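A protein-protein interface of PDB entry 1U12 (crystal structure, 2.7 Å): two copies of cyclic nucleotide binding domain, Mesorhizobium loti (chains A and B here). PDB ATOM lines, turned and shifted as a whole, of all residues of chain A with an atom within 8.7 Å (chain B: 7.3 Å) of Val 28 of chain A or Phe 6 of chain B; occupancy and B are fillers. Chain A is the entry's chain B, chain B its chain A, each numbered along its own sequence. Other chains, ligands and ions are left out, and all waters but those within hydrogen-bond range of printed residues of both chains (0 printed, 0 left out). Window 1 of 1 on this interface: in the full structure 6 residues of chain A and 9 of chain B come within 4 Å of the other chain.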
ATOM      1  N   PHE A   6      20.838 -12.433  12.060  1.00  0.00           N
ATOM      2  CA  PHE A   6      20.303 -11.992  13.328  1.00  0.00           C
ATOM      3  C   PHE A   6      18.791 -11.812  13.365  1.00  0.00           C
ATOM      4  O   PHE A   6      18.138 -12.277  14.293  1.00  0.00           O
ATOM      5  CB  PHE A   6      20.946 -10.676  13.736  1.00  0.00           C
ATOM      6  CG  PHE A   6      20.584 -10.251  15.111  1.00  0.00           C
ATOM      7  CD1 PHE A   6      21.147 -10.891  16.212  1.00  0.00           C
ATOM      8  CD2 PHE A   6      19.638  -9.255  15.317  1.00  0.00           C
ATOM      9  CE1 PHE A   6      20.769 -10.543  17.504  1.00  0.00           C
ATOM     10  CE2 PHE A   6      19.248  -8.899  16.609  1.00  0.00           C
ATOM     11  CZ  PHE A   6      19.815  -9.544  17.705  1.00  0.00           C
ATOM     12  N   VAL A   7      18.232 -11.125  12.375  1.00  0.00           N
ATOM     13  CA  VAL A   7      16.800 -10.895  12.375  1.00  0.00           C
ATOM     14  C   VAL A   7      16.070 -12.188  12.064  1.00  0.00           C
ATOM     15  O   VAL A   7      15.066 -12.514  12.698  1.00  0.00           O
ATOM     16  CB  VAL A   7      16.419  -9.783  11.382  1.00  0.00           C
ATOM     17  CG1 VAL A   7      17.358  -8.599  11.516  1.00  0.00           C
ATOM     18  CG2 VAL A   7      16.434 -10.302   9.959  1.00  0.00           C
ATOM     19  N   ASN A   9      17.085 -15.208  12.675  1.00  0.00           N
ATOM     20  CA  ASN A   9      17.202 -15.954  13.922  1.00  0.00           C
ATOM     21  C   ASN A   9      16.286 -15.408  15.003  1.00  0.00           C
ATOM     22  O   ASN A   9      15.731 -16.162  15.799  1.00  0.00           O
ATOM     23  CB  ASN A   9      18.654 -15.966  14.380  1.00  0.00           C
ATOM     24  CG  ASN A   9      19.514 -16.888  13.529  1.00  0.00           C
ATOM     25  OD1 ASN A   9      20.737 -16.890  13.632  1.00  0.00           O
ATOM     26  ND2 ASN A   9      18.867 -17.678  12.678  1.00  0.00           N
ATOM     27  N   TRP A  10      16.151 -14.086  15.041  1.00  0.00           N
ATOM     28  CA  TRP A  10      15.258 -13.439  15.970  1.00  0.00           C
ATOM     29  C   TRP A  10      13.840 -13.964  15.767  1.00  0.00           C
ATOM     30  O   TRP A  10      13.210 -14.453  16.707  1.00  0.00           O
ATOM     31  CB  TRP A  10      15.285 -11.926  15.769  1.00  0.00           C
ATOM     32  CG  TRP A  10      14.316 -11.216  16.687  1.00  0.00           C
ATOM     33  CD1 TRP A  10      12.990 -11.053  16.497  1.00  0.00           C
ATOM     34  CD2 TRP A  10      14.646 -10.597  17.935  1.00  0.00           C
ATOM     35  NE1 TRP A  10      12.435 -10.394  17.567  1.00  0.00           N
ATOM     36  CE2 TRP A  10      13.429 -10.104  18.467  1.00  0.00           C
ATOM     37  CE3 TRP A  10      15.830 -10.421  18.669  1.00  0.00           C
ATOM     38  CZ2 TRP A  10      13.366  -9.450  19.698  1.00  0.00           C
ATOM     39  CZ3 TRP A  10      15.768  -9.769  19.891  1.00  0.00           C
ATOM     40  CH2 TRP A  10      14.544  -9.293  20.395  1.00  0.00           C
ATOM     41  N   VAL A  13      13.273 -17.608  16.713  1.00  0.00           N
ATOM     42  CA  VAL A  13      13.189 -17.757  18.165  1.00  0.00           C
ATOM     43  C   VAL A  13      11.887 -17.153  18.717  1.00  0.00           C
ATOM     44  O   VAL A  13      11.290 -17.699  19.648  1.00  0.00           O
ATOM     45  CB  VAL A  13      14.385 -17.081  18.868  1.00  0.00           C
ATOM     46  CG1 VAL A  13      14.166 -17.007  20.374  1.00  0.00           C
ATOM     47  CG2 VAL A  13      15.685 -17.814  18.545  1.00  0.00           C
ATOM     48  N   LEU A  22       8.777 -13.185  27.260  1.00  0.00           N
ATOM     49  CA  LEU A  22      10.124 -12.655  27.455  1.00  0.00           C
ATOM     50  C   LEU A  22      10.324 -11.312  26.761  1.00  0.00           C
ATOM     51  O   LEU A  22       9.748 -11.056  25.704  1.00  0.00           O
ATOM     52  CB  LEU A  22      11.161 -13.655  26.934  1.00  0.00           C
ATOM     53  CG  LEU A  22      11.182 -15.042  27.576  1.00  0.00           C
ATOM     54  CD1 LEU A  22      12.233 -15.910  26.891  1.00  0.00           C
ATOM     55  CD2 LEU A  22      11.476 -14.895  29.064  1.00  0.00           C
ATOM     56  N   GLY A  23      11.141 -10.455  27.362  1.00  0.00           N
ATOM     57  CA  GLY A  23      11.410  -9.157  26.767  1.00  0.00           C
ATOM     58  C   GLY A  23      12.445  -9.265  25.655  1.00  0.00           C
ATOM     59  O   GLY A  23      13.016 -10.335  25.441  1.00  0.00           O
ATOM     60  N   PRO A  24      12.708  -8.174  24.920  1.00  0.00           N
ATOM     61  CA  PRO A  24      13.695  -8.211  23.835  1.00  0.00           C
ATOM     62  C   PRO A  24      15.106  -8.556  24.314  1.00  0.00           C
ATOM     63  O   PRO A  24      15.780  -9.410  23.732  1.00  0.00           O
ATOM     64  CB  PRO A  24      13.607  -6.804  23.251  1.00  0.00           C
ATOM     65  CG  PRO A  24      12.163  -6.459  23.453  1.00  0.00           C
ATOM     66  CD  PRO A  24      11.943  -6.916  24.879  1.00  0.00           C
ATOM     67  N   ALA A  25      15.547  -7.891  25.374  1.00  0.00           N
ATOM     68  CA  ALA A  25      16.875  -8.134  25.920  1.00  0.00           C
ATOM     69  C   ALA A  25      17.147  -9.618  26.129  1.00  0.00           C
ATOM     70  O   ALA A  25      18.287 -10.072  26.002  1.00  0.00           O
ATOM     71  CB  ALA A  25      17.038  -7.392  27.234  1.00  0.00           C
ATOM     72  N   VAL A  26      16.101 -10.370  26.453  1.00  0.00           N
ATOM     73  CA  VAL A  26      16.237 -11.802  26.678  1.00  0.00           C
ATOM     74  C   VAL A  26      16.251 -12.605  25.362  1.00  0.00           C
ATOM     75  O   VAL A  26      16.942 -13.616  25.263  1.00  0.00           O
ATOM     76  CB  VAL A  26      15.107 -12.306  27.601  1.00  0.00           C
ATOM     77  CG1 VAL A  26      15.368 -13.751  28.024  1.00  0.00           C
ATOM     78  CG2 VAL A  26      15.005 -11.405  28.813  1.00  0.00           C
ATOM     79  N   LEU A  27      15.490 -12.171  24.357  1.00  0.00           N
ATOM     80  CA  LEU A  27      15.486 -12.883  23.077  1.00  0.00           C
ATOM     81  C   LEU A  27      16.862 -12.726  22.435  1.00  0.00           C
ATOM     82  O   LEU A  27      17.355 -13.629  21.761  1.00  0.00           O
ATOM     83  CB  LEU A  27      14.416 -12.329  22.128  1.00  0.00           C
ATOM     84  CG  LEU A  27      12.960 -12.777  22.297  1.00  0.00           C
ATOM     85  CD1 LEU A  27      12.124 -12.202  21.153  1.00  0.00           C
ATOM     86  CD2 LEU A  27      12.867 -14.287  22.290  1.00  0.00           C
ATOM     87  N   VAL A  28      17.481 -11.572  22.656  1.00  0.00           N
ATOM     88  CA  VAL A  28      18.798 -11.305  22.109  1.00  0.00           C
ATOM     89  C   VAL A  28      19.783 -12.302  22.696  1.00  0.00           C
ATOM     90  O   VAL A  28      20.736 -12.729  22.031  1.00  0.00           O
ATOM     91  CB  VAL A  28      19.252  -9.871  22.452  1.00  0.00           C
ATOM     92  CG1 VAL A  28      20.723  -9.686  22.078  1.00  0.00           C
ATOM     93  CG2 VAL A  28      18.375  -8.857  21.704  1.00  0.00           C
ATOM     94  N   GLU A  29      19.531 -12.674  23.948  1.00  0.00           N
ATOM     95  CA  GLU A  29      20.366 -13.626  24.670  1.00  0.00           C
ATOM     96  C   GLU A  29      20.200 -15.051  24.144  1.00  0.00           C
ATOM     97  O   GLU A  29      21.179 -15.772  23.921  1.00  0.00           O
ATOM     98  CB  GLU A  29      20.041 -13.554  26.166  1.00  0.00           C
ATOM     99  CG  GLU A  29      20.567 -12.287  26.809  1.00  0.00           C
ATOM    100  CD  GLU A  29      22.019 -12.048  26.421  1.00  0.00           C
ATOM    101  OE1 GLU A  29      22.843 -12.965  26.639  1.00  0.00           O
ATOM    102  OE2 GLU A  29      22.340 -10.960  25.888  1.00  0.00           O
ATOM    103  N   ILE A  30      18.952 -15.451  23.947  1.00  0.00           N
ATOM    104  CA  ILE A  30      18.642 -16.774  23.423  1.00  0.00           C
ATOM    105  C   ILE A  30      19.268 -16.926  22.028  1.00  0.00           C
ATOM    106  O   ILE A  30      19.800 -17.995  21.683  1.00  0.00           O
ATOM    107  CB  ILE A  30      17.113 -16.963  23.300  1.00  0.00           C
ATOM    108  CG1 ILE A  30      16.460 -16.751  24.676  1.00  0.00           C
ATOM    109  CG2 ILE A  30      16.800 -18.313  22.663  1.00  0.00           C
ATOM    110  CD1 ILE A  30      15.632 -17.909  25.183  1.00  0.00           C
ATOM    111  N   VAL A  31      19.200 -15.841  21.248  1.00  0.00           N
ATOM    112  CA  VAL A  31      19.712 -15.798  19.881  1.00  0.00           C
ATOM    113  C   VAL A  31      21.214 -15.997  19.813  1.00  0.00           C
ATOM    114  O   VAL A  31      21.698 -16.866  19.086  1.00  0.00           O
ATOM    115  CB  VAL A  31      19.345 -14.455  19.186  1.00  0.00           C
ATOM    116  CG1 VAL A  31      20.121 -14.297  17.880  1.00  0.00           C
ATOM    117  CG2 VAL A  31      17.853 -14.415  18.906  1.00  0.00           C
ATOM    118  N   ARG A  32      21.949 -15.185  20.561  1.00  0.00           N
ATOM    119  CA  ARG A  32      23.401 -15.296  20.587  1.00  0.00           C
ATOM    120  C   ARG A  32      23.789 -16.714  20.996  1.00  0.00           C
ATOM    121  O   ARG A  32      24.761 -17.276  20.503  1.00  0.00           O
ATOM    122  CB  ARG A  32      23.979 -14.298  21.591  1.00  0.00           C
ATOM    123  CG  ARG A  32      23.529 -12.867  21.370  1.00  0.00           C
ATOM    124  CD  ARG A  32      24.258 -11.936  22.315  1.00  0.00           C
ATOM    125  NE  ARG A  32      25.704 -12.093  22.184  1.00  0.00           N
ATOM    126  CZ  ARG A  32      26.562 -11.931  23.186  1.00  0.00           C
ATOM    127  NH1 ARG A  32      26.109 -11.605  24.393  1.00  0.00           N
ATOM    128  NH2 ARG A  32      27.863 -12.112  22.989  1.00  0.00           N
ATOM    129  N   ALA A  33      23.002 -17.298  21.887  1.00  0.00           N
ATOM    130  CA  ALA A  33      23.277 -18.634  22.384  1.00  0.00           C
ATOM    131  C   ALA A  33      23.050 -19.759  21.368  1.00  0.00           C
ATOM    132  O   ALA A  33      23.435 -20.906  21.608  1.00  0.00           O
ATOM    133  CB  ALA A  33      22.449 -18.886  23.635  1.00  0.00           C
ATOM    134  N   LEU A  34      22.439 -19.423  20.234  1.00  0.00           N
ATOM    135  CA  LEU A  34      22.144 -20.399  19.184  1.00  0.00           C
ATOM    136  C   LEU A  34      23.401 -20.935  18.507  1.00  0.00           C
ATOM    137  O   LEU A  34      24.267 -20.167  18.084  1.00  0.00           O
ATOM    138  CB  LEU A  34      21.226 -19.772  18.124  1.00  0.00           C
ATOM    139  CG  LEU A  34      19.846 -19.264  18.571  1.00  0.00           C
ATOM    140  CD1 LEU A  34      19.132 -18.629  17.391  1.00  0.00           C
ATOM    141  CD2 LEU A  34      19.024 -20.403  19.146  1.00  0.00           C
ATOM    142  N   LEU A 113      20.422 -18.605  31.861  1.00  0.00           N
ATOM    143  CA  LEU A 113      19.862 -17.317  31.501  1.00  0.00           C
ATOM    144  C   LEU A 113      18.864 -16.950  32.595  1.00  0.00           C
ATOM    145  O   LEU A 113      18.773 -15.796  33.001  1.00  0.00           O
ATOM    146  CB  LEU A 113      19.155 -17.388  30.153  1.00  0.00           C
ATOM    147  CG  LEU A 113      18.273 -16.180  29.825  1.00  0.00           C
ATOM    148  CD1 LEU A 113      19.046 -14.881  30.045  1.00  0.00           C
ATOM    149  CD2 LEU A 113      17.782 -16.290  28.380  1.00  0.00           C
ATOM    150  N   ARG B   2       6.948  -3.334  22.639  1.00  0.00           N
ATOM    151  CA  ARG B   2       6.788  -4.569  21.812  1.00  0.00           C
ATOM    152  C   ARG B   2       8.136  -5.152  21.370  1.00  0.00           C
ATOM    153  O   ARG B   2       9.202  -4.607  21.676  1.00  0.00           O
ATOM    154  CB  ARG B   2       5.914  -4.267  20.581  1.00  0.00           C
ATOM    155  N   ARG B   3       8.072  -6.273  20.654  1.00  0.00           N
ATOM    156  CA  ARG B   3       9.261  -6.951  20.148  1.00  0.00           C
ATOM    157  C   ARG B   3       9.342  -6.703  18.649  1.00  0.00           C
ATOM    158  O   ARG B   3      10.371  -6.942  18.021  1.00  0.00           O
ATOM    159  CB  ARG B   3       9.177  -8.457  20.437  1.00  0.00           C
ATOM    160  N   GLY B   4       8.237  -6.220  18.087  1.00  0.00           N
ATOM    161  CA  GLY B   4       8.182  -5.933  16.666  1.00  0.00           C
ATOM    162  C   GLY B   4       8.970  -4.684  16.331  1.00  0.00           C
ATOM    163  O   GLY B   4       9.751  -4.673  15.381  1.00  0.00           O
ATOM    164  N   ASP B   5       8.773  -3.627  17.111  1.00  0.00           N
ATOM    165  CA  ASP B   5       9.486  -2.378  16.878  1.00  0.00           C
ATOM    166  C   ASP B   5      10.955  -2.492  17.278  1.00  0.00           C
ATOM    167  O   ASP B   5      11.772  -1.641  16.917  1.00  0.00           O
ATOM    168  CB  ASP B   5       8.829  -1.227  17.649  1.00  0.00           C
ATOM    169  CG  ASP B   5       7.386  -0.996  17.236  1.00  0.00           C
ATOM    170  OD1 ASP B   5       7.109  -0.994  16.018  1.00  0.00           O
ATOM    171  OD2 ASP B   5       6.531  -0.806  18.126  1.00  0.00           O
ATOM    172  N   PHE B   6      11.291  -3.541  18.027  1.00  0.00           N
ATOM    173  CA  PHE B   6      12.673  -3.751  18.447  1.00  0.00           C
ATOM    174  C   PHE B   6      13.468  -4.184  17.221  1.00  0.00           C
ATOM    175  O   PHE B   6      14.570  -3.695  16.958  1.00  0.00           O
ATOM    176  CB  PHE B   6      12.766  -4.857  19.501  1.00  0.00           C
ATOM    177  CG  PHE B   6      14.145  -5.024  20.073  1.00  0.00           C
ATOM    178  CD1 PHE B   6      14.527  -4.326  21.216  1.00  0.00           C
ATOM    179  CD2 PHE B   6      15.089  -5.819  19.424  1.00  0.00           C
ATOM    180  CE1 PHE B   6      15.838  -4.410  21.705  1.00  0.00           C
ATOM    181  CE2 PHE B   6      16.394  -5.910  19.897  1.00  0.00           C
ATOM    182  CZ  PHE B   6      16.772  -5.203  21.041  1.00  0.00           C
ATOM    183  N   VAL B   7      12.882  -5.113  16.477  1.00  0.00           N
ATOM    184  CA  VAL B   7      13.503  -5.657  15.283  1.00  0.00           C
ATOM    185  C   VAL B   7      13.734  -4.600  14.216  1.00  0.00           C
ATOM    186  O   VAL B   7      14.758  -4.616  13.528  1.00  0.00           O
ATOM    187  CB  VAL B   7      12.635  -6.774  14.678  1.00  0.00           C
ATOM    188  CG1 VAL B   7      13.344  -7.400  13.482  1.00  0.00           C
ATOM    189  CG2 VAL B   7      12.331  -7.816  15.741  1.00  0.00           C
ATOM    190  N   ARG B   8      12.786  -3.684  14.067  1.00  0.00           N
ATOM    191  CA  ARG B   8      12.944  -2.656  13.056  1.00  0.00           C
ATOM    192  C   ARG B   8      13.817  -1.518  13.566  1.00  0.00           C
ATOM    193  O   ARG B   8      14.412  -0.788  12.777  1.00  0.00           O
ATOM    194  CB  ARG B   8      11.573  -2.151  12.570  1.00  0.00           C
ATOM    195  CG  ARG B   8      10.711  -1.431  13.588  1.00  0.00           C
ATOM    196  CD  ARG B   8      11.232  -0.028  13.862  1.00  0.00           C
ATOM    197  NE  ARG B   8      10.329   0.734  14.722  1.00  0.00           N
ATOM    198  CZ  ARG B   8       9.178   1.251  14.307  1.00  0.00           C
ATOM    199  NH1 ARG B   8       8.799   1.089  13.043  1.00  0.00           N
ATOM    200  NH2 ARG B   8       8.407   1.921  15.154  1.00  0.00           N
ATOM    201  N   ASN B   9      13.899  -1.365  14.884  1.00  0.00           N
ATOM    202  CA  ASN B   9      14.747  -0.320  15.453  1.00  0.00           C
ATOM    203  C   ASN B   9      16.171  -0.858  15.350  1.00  0.00           C
ATOM    204  O   ASN B   9      17.151  -0.108  15.355  1.00  0.00           O
ATOM    205  CB  ASN B   9      14.360  -0.027  16.918  1.00  0.00           C
ATOM    206  CG  ASN B   9      13.152   0.904  17.031  1.00  0.00           C
ATOM    207  OD1 ASN B   9      12.542   1.271  16.030  1.00  0.00           O
ATOM    208  ND2 ASN B   9      12.804   1.285  18.254  1.00  0.00           N
ATOM    209  N   TRP B  10      16.263  -2.177  15.239  1.00  0.00           N
ATOM    210  CA  TRP B  10      17.541  -2.852  15.102  1.00  0.00           C
ATOM    211  C   TRP B  10      18.009  -2.707  13.664  1.00  0.00           C
ATOM    212  O   TRP B  10      19.158  -2.344  13.414  1.00  0.00           O
ATOM    213  CB  TRP B  10      17.401  -4.329  15.458  1.00  0.00           C
ATOM    214  CG  TRP B  10      18.621  -5.124  15.144  1.00  0.00           C
ATOM    215  CD1 TRP B  10      18.995  -5.631  13.921  1.00  0.00           C
ATOM    216  CD2 TRP B  10      19.657  -5.470  16.055  1.00  0.00           C
ATOM    217  NE1 TRP B  10      20.207  -6.270  14.027  1.00  0.00           N
ATOM    218  CE2 TRP B  10      20.637  -6.183  15.327  1.00  0.00           C
ATOM    219  CE3 TRP B  10      19.857  -5.247  17.421  1.00  0.00           C
ATOM    220  CZ2 TRP B  10      21.800  -6.674  15.921  1.00  0.00           C
ATOM    221  CZ3 TRP B  10      21.012  -5.734  18.015  1.00  0.00           C
ATOM    222  CH2 TRP B  10      21.972  -6.441  17.264  1.00  0.00           C
ATOM    223  N   GLN B  11      17.114  -2.996  12.720  1.00  0.00           N
ATOM    224  CA  GLN B  11      17.439  -2.878  11.301  1.00  0.00           C
ATOM    225  C   GLN B  11      17.695  -1.426  10.900  1.00  0.00           C
ATOM    226  O   GLN B  11      18.521  -1.157  10.025  1.00  0.00           O
ATOM    227  CB  GLN B  11      16.319  -3.465  10.452  1.00  0.00           C
ATOM    228  CG  GLN B  11      16.076  -4.942  10.725  1.00  0.00           C
ATOM    229  CD  GLN B  11      14.894  -5.487   9.943  1.00  0.00           C
ATOM    230  OE1 GLN B  11      15.033  -5.977   8.827  1.00  0.00           O
ATOM    231  NE2 GLN B  11      13.632  -5.491  10.361  1.00  0.00           N
ATOM    232  N   LEU B  12      16.991  -0.494  11.539  1.00  0.00           N
ATOM    233  CA  LEU B  12      17.171   0.927  11.295  1.00  0.00           C
ATOM    234  C   LEU B  12      18.622   1.270  11.580  1.00  0.00           C
ATOM    235  O   LEU B  12      19.355   1.743  10.711  1.00  0.00           O
ATOM    236  CB  LEU B  12      16.235   1.755  12.191  1.00  0.00           C
ATOM    237  CG  LEU B  12      15.428   2.920  11.569  1.00  0.00           C
ATOM    238  CD1 LEU B  12      16.364   3.879  10.832  1.00  0.00           C
ATOM    239  CD2 LEU B  12      14.346   2.379  10.644  1.00  0.00           C
ATOM    240  N   PRO B  24      26.415  -8.037  17.292  1.00  0.00           N
ATOM    241  CA  PRO B  24      25.047  -7.783  17.738  1.00  0.00           C
ATOM    242  C   PRO B  24      24.994  -7.279  19.165  1.00  0.00           C
ATOM    243  O   PRO B  24      24.264  -6.361  19.545  1.00  0.00           O
ATOM    244  CB  PRO B  24      24.377  -9.118  17.541  1.00  0.00           C
ATOM    245  CG  PRO B  24      24.800  -9.371  16.135  1.00  0.00           C
ATOM    246  CD  PRO B  24      26.107  -8.632  15.957  1.00  0.00           C
ATOM    247  N   ALA B  25      25.842  -7.930  19.936  1.00  0.00           N
ATOM    248  CA  ALA B  25      26.009  -7.670  21.353  1.00  0.00           C
ATOM    249  C   ALA B  25      26.083  -6.166  21.597  1.00  0.00           C
ATOM    250  O   ALA B  25      25.687  -5.693  22.664  1.00  0.00           O
ATOM    251  CB  ALA B  25      27.267  -8.362  21.872  1.00  0.00           C
ATOM    252  N   LEU B  27      25.036  -3.552  19.081  1.00  0.00           N
ATOM    253  CA  LEU B  27      23.885  -2.873  18.511  1.00  0.00           C
ATOM    254  C   LEU B  27      22.662  -2.995  19.422  1.00  0.00           C
ATOM    255  O   LEU B  27      21.765  -2.155  19.390  1.00  0.00           O
ATOM    256  CB  LEU B  27      23.588  -3.444  17.124  1.00  0.00           C
ATOM    257  CG  LEU B  27      24.801  -3.476  16.182  1.00  0.00           C
ATOM    258  CD1 LEU B  27      24.439  -4.155  14.878  1.00  0.00           C
ATOM    259  CD2 LEU B  27      25.296  -2.071  15.925  1.00  0.00           C
ATOM    260  N   VAL B  28      22.633  -4.044  20.238  1.00  0.00           N
ATOM    261  CA  VAL B  28      21.523  -4.259  21.152  1.00  0.00           C
ATOM    262  C   VAL B  28      21.515  -3.117  22.132  1.00  0.00           C
ATOM    263  O   VAL B  28      20.462  -2.561  22.451  1.00  0.00           O
ATOM    264  CB  VAL B  28      21.684  -5.557  21.955  1.00  0.00           C
ATOM    265  CG1 VAL B  28      20.552  -5.680  22.981  1.00  0.00           C
ATOM    266  CG2 VAL B  28      21.694  -6.742  21.014  1.00  0.00           C
ATOM    267  N   GLU B  29      22.708  -2.776  22.609  1.00  0.00           N
ATOM    268  CA  GLU B  29      22.876  -1.699  23.565  1.00  0.00           C
ATOM    269  C   GLU B  29      22.425  -0.368  22.990  1.00  0.00           C
ATOM    270  O   GLU B  29      21.690   0.373  23.650  1.00  0.00           O
ATOM    271  CB  GLU B  29      24.334  -1.597  23.999  1.00  0.00           C
ATOM    272  CG  GLU B  29      24.773  -2.709  24.918  1.00  0.00           C
ATOM    273  CD  GLU B  29      23.780  -2.947  26.045  1.00  0.00           C
ATOM    274  OE1 GLU B  29      23.393  -1.971  26.728  1.00  0.00           O
ATOM    275  OE2 GLU B  29      23.389  -4.117  26.246  1.00  0.00           O
ATOM    276  N   VAL B  31      20.335   0.293  20.530  1.00  0.00           N
ATOM    277  CA  VAL B  31      18.883   0.268  20.414  1.00  0.00           C
ATOM    278  C   VAL B  31      18.170   0.586  21.718  1.00  0.00           C
ATOM    279  O   VAL B  31      17.037   1.081  21.664  1.00  0.00           O
ATOM    280  CB  VAL B  31      18.406  -1.109  19.888  1.00  0.00           C
ATOM    281  CG1 VAL B  31      16.881  -1.186  19.926  1.00  0.00           C
ATOM    282  CG2 VAL B  31      18.933  -1.357  18.478  1.00  0.00           C
ATOM    283  N   ARG B  32      18.773   0.335  22.891  1.00  0.00           N
ATOM    284  CA  ARG B  32      18.067   0.574  24.169  1.00  0.00           C
ATOM    285  C   ARG B  32      18.422   1.916  24.820  1.00  0.00           C
ATOM    286  O   ARG B  32      17.909   2.253  25.894  1.00  0.00           O
ATOM    287  CB  ARG B  32      18.346  -0.561  25.140  1.00  0.00           C
ATOM    288  CG  ARG B  32      17.739  -1.897  24.705  1.00  0.00           C
ATOM    289  CD  ARG B  32      16.239  -1.790  24.479  1.00  0.00           C
ATOM    290  NE  ARG B  32      15.544  -2.991  24.931  1.00  0.00           N
ATOM    291  CZ  ARG B  32      14.227  -3.164  24.857  1.00  0.00           C
ATOM    292  NH1 ARG B  32      13.462  -2.210  24.347  1.00  0.00           N
ATOM    293  NH2 ARG B  32      13.682  -4.291  25.294  1.00  0.00           N
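The backbone carbonyl oxygen of Val 7 of chain B lies close to the side-chain amide nitrogen of Gln 11 of chain B (3.5 Å).
Among the printed residues, pairs that only touch across the chains: Trp 10 of chain A with Val 7 of chain B (3.2 Å), Pro 24 of chain A with Arg 32 of chain B (3.2 Å), Phe 6 of chain A with Trp 10 of chain B (3.2 Å), Val 28 of chain A with Val 28 of chain B (3.3 Å), Pro 24 of chain A with Phe 6 of chain B (3.3 Å), Trp 10 of chain A with Phe 6 of chain B (3.6 Å), Arg 32 of chain A with Ala 25 of chain B (3.9 Å), Phe 6 of chain A with Pro 24 of chain B (3.9 Å), Pro 24 of chain A with Arg 2 of chain B (3.9 Å), Val 7 of chain A with Gln 11 of chain B (3.96 Å) and Val 28 of chain A with Phe 6 of chain B (3.98 Å).
Of the printed residues of chain B, Trp 10 of chain A touches Phe 6 and Val 7.
Of the printed residues of chain B, Val 28 of chain A touches Phe 6 (3.98 Å) and Val 28 (3.3 Å).
Of the printed residues of chain B, Arg 32 of chain A touches Ala 25 (3.9 Å).
Printed residues of chain A within 4 Å of Arg 2 of chain B: Pro 24 (3.9 Å).
Gly 4 of chain B touches none of the printed residues of chain A.
Of the printed residues of chain A, Phe 6 of chain B touches Trp 10, Pro 24 and Val 28.
The nearest printed residue of chain B that does not touch Val 28 of chain A is Pro 24 of chain B (5.5 Å).
The nearest printed residue of chain A that does not touch Phe 6 of chain B is Ala 25 of chain A (5.1 Å).
Of the 18 printed residues of chain B, 9 touch a printed residue of chain A.
Printed residues of chain B that touch a printed residue of chain A: Arg 2, Phe 6, Val 7, Trp 10, Gln 11, Pro 24, Ala 25, Val 28 and Arg 32.
Hydrophobic or aromatic side chains of chain B within 4 Å of the printed part of chain A: Phe 6, Val 7, Trp 10, Pro 24, Ala 25 and Val 28.
Of the 19 printed residues of chain A, 6 touch a printed residue of chain B.
Hydrophobic or aromatic side chains of chain A within 4 Å of the printed part of chain B: Phe 6, Val 7, Trp 10, Pro 24 and Val 28.
Along chain A the printed residues that touch a printed residue of chain B span positions 6 to 32.
Among the printed residues, no Asp or Glu carboxylate lies within 4 Å of a Lys or Arg side-chain nitrogen of the other chain.
Phe 6 of chain A touches Pro 24 of chain B, and with the chains exchanged Pro 24 of chain A touches Phe 6 of chain B.
Val 28 of chain A touches Phe 6 of chain B, but with the chains exchanged Phe 6 of chain A does not touch Val 28 of chain B (4.7 Å).
Val 28 of chain B touches its own counterpart, Val 28 of chain A.
Arg 32 of chain A touches Ala 25 of chain B, but with the chains exchanged Ala 25 of chain A does not touch Arg 32 of chain B (4.1 Å).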
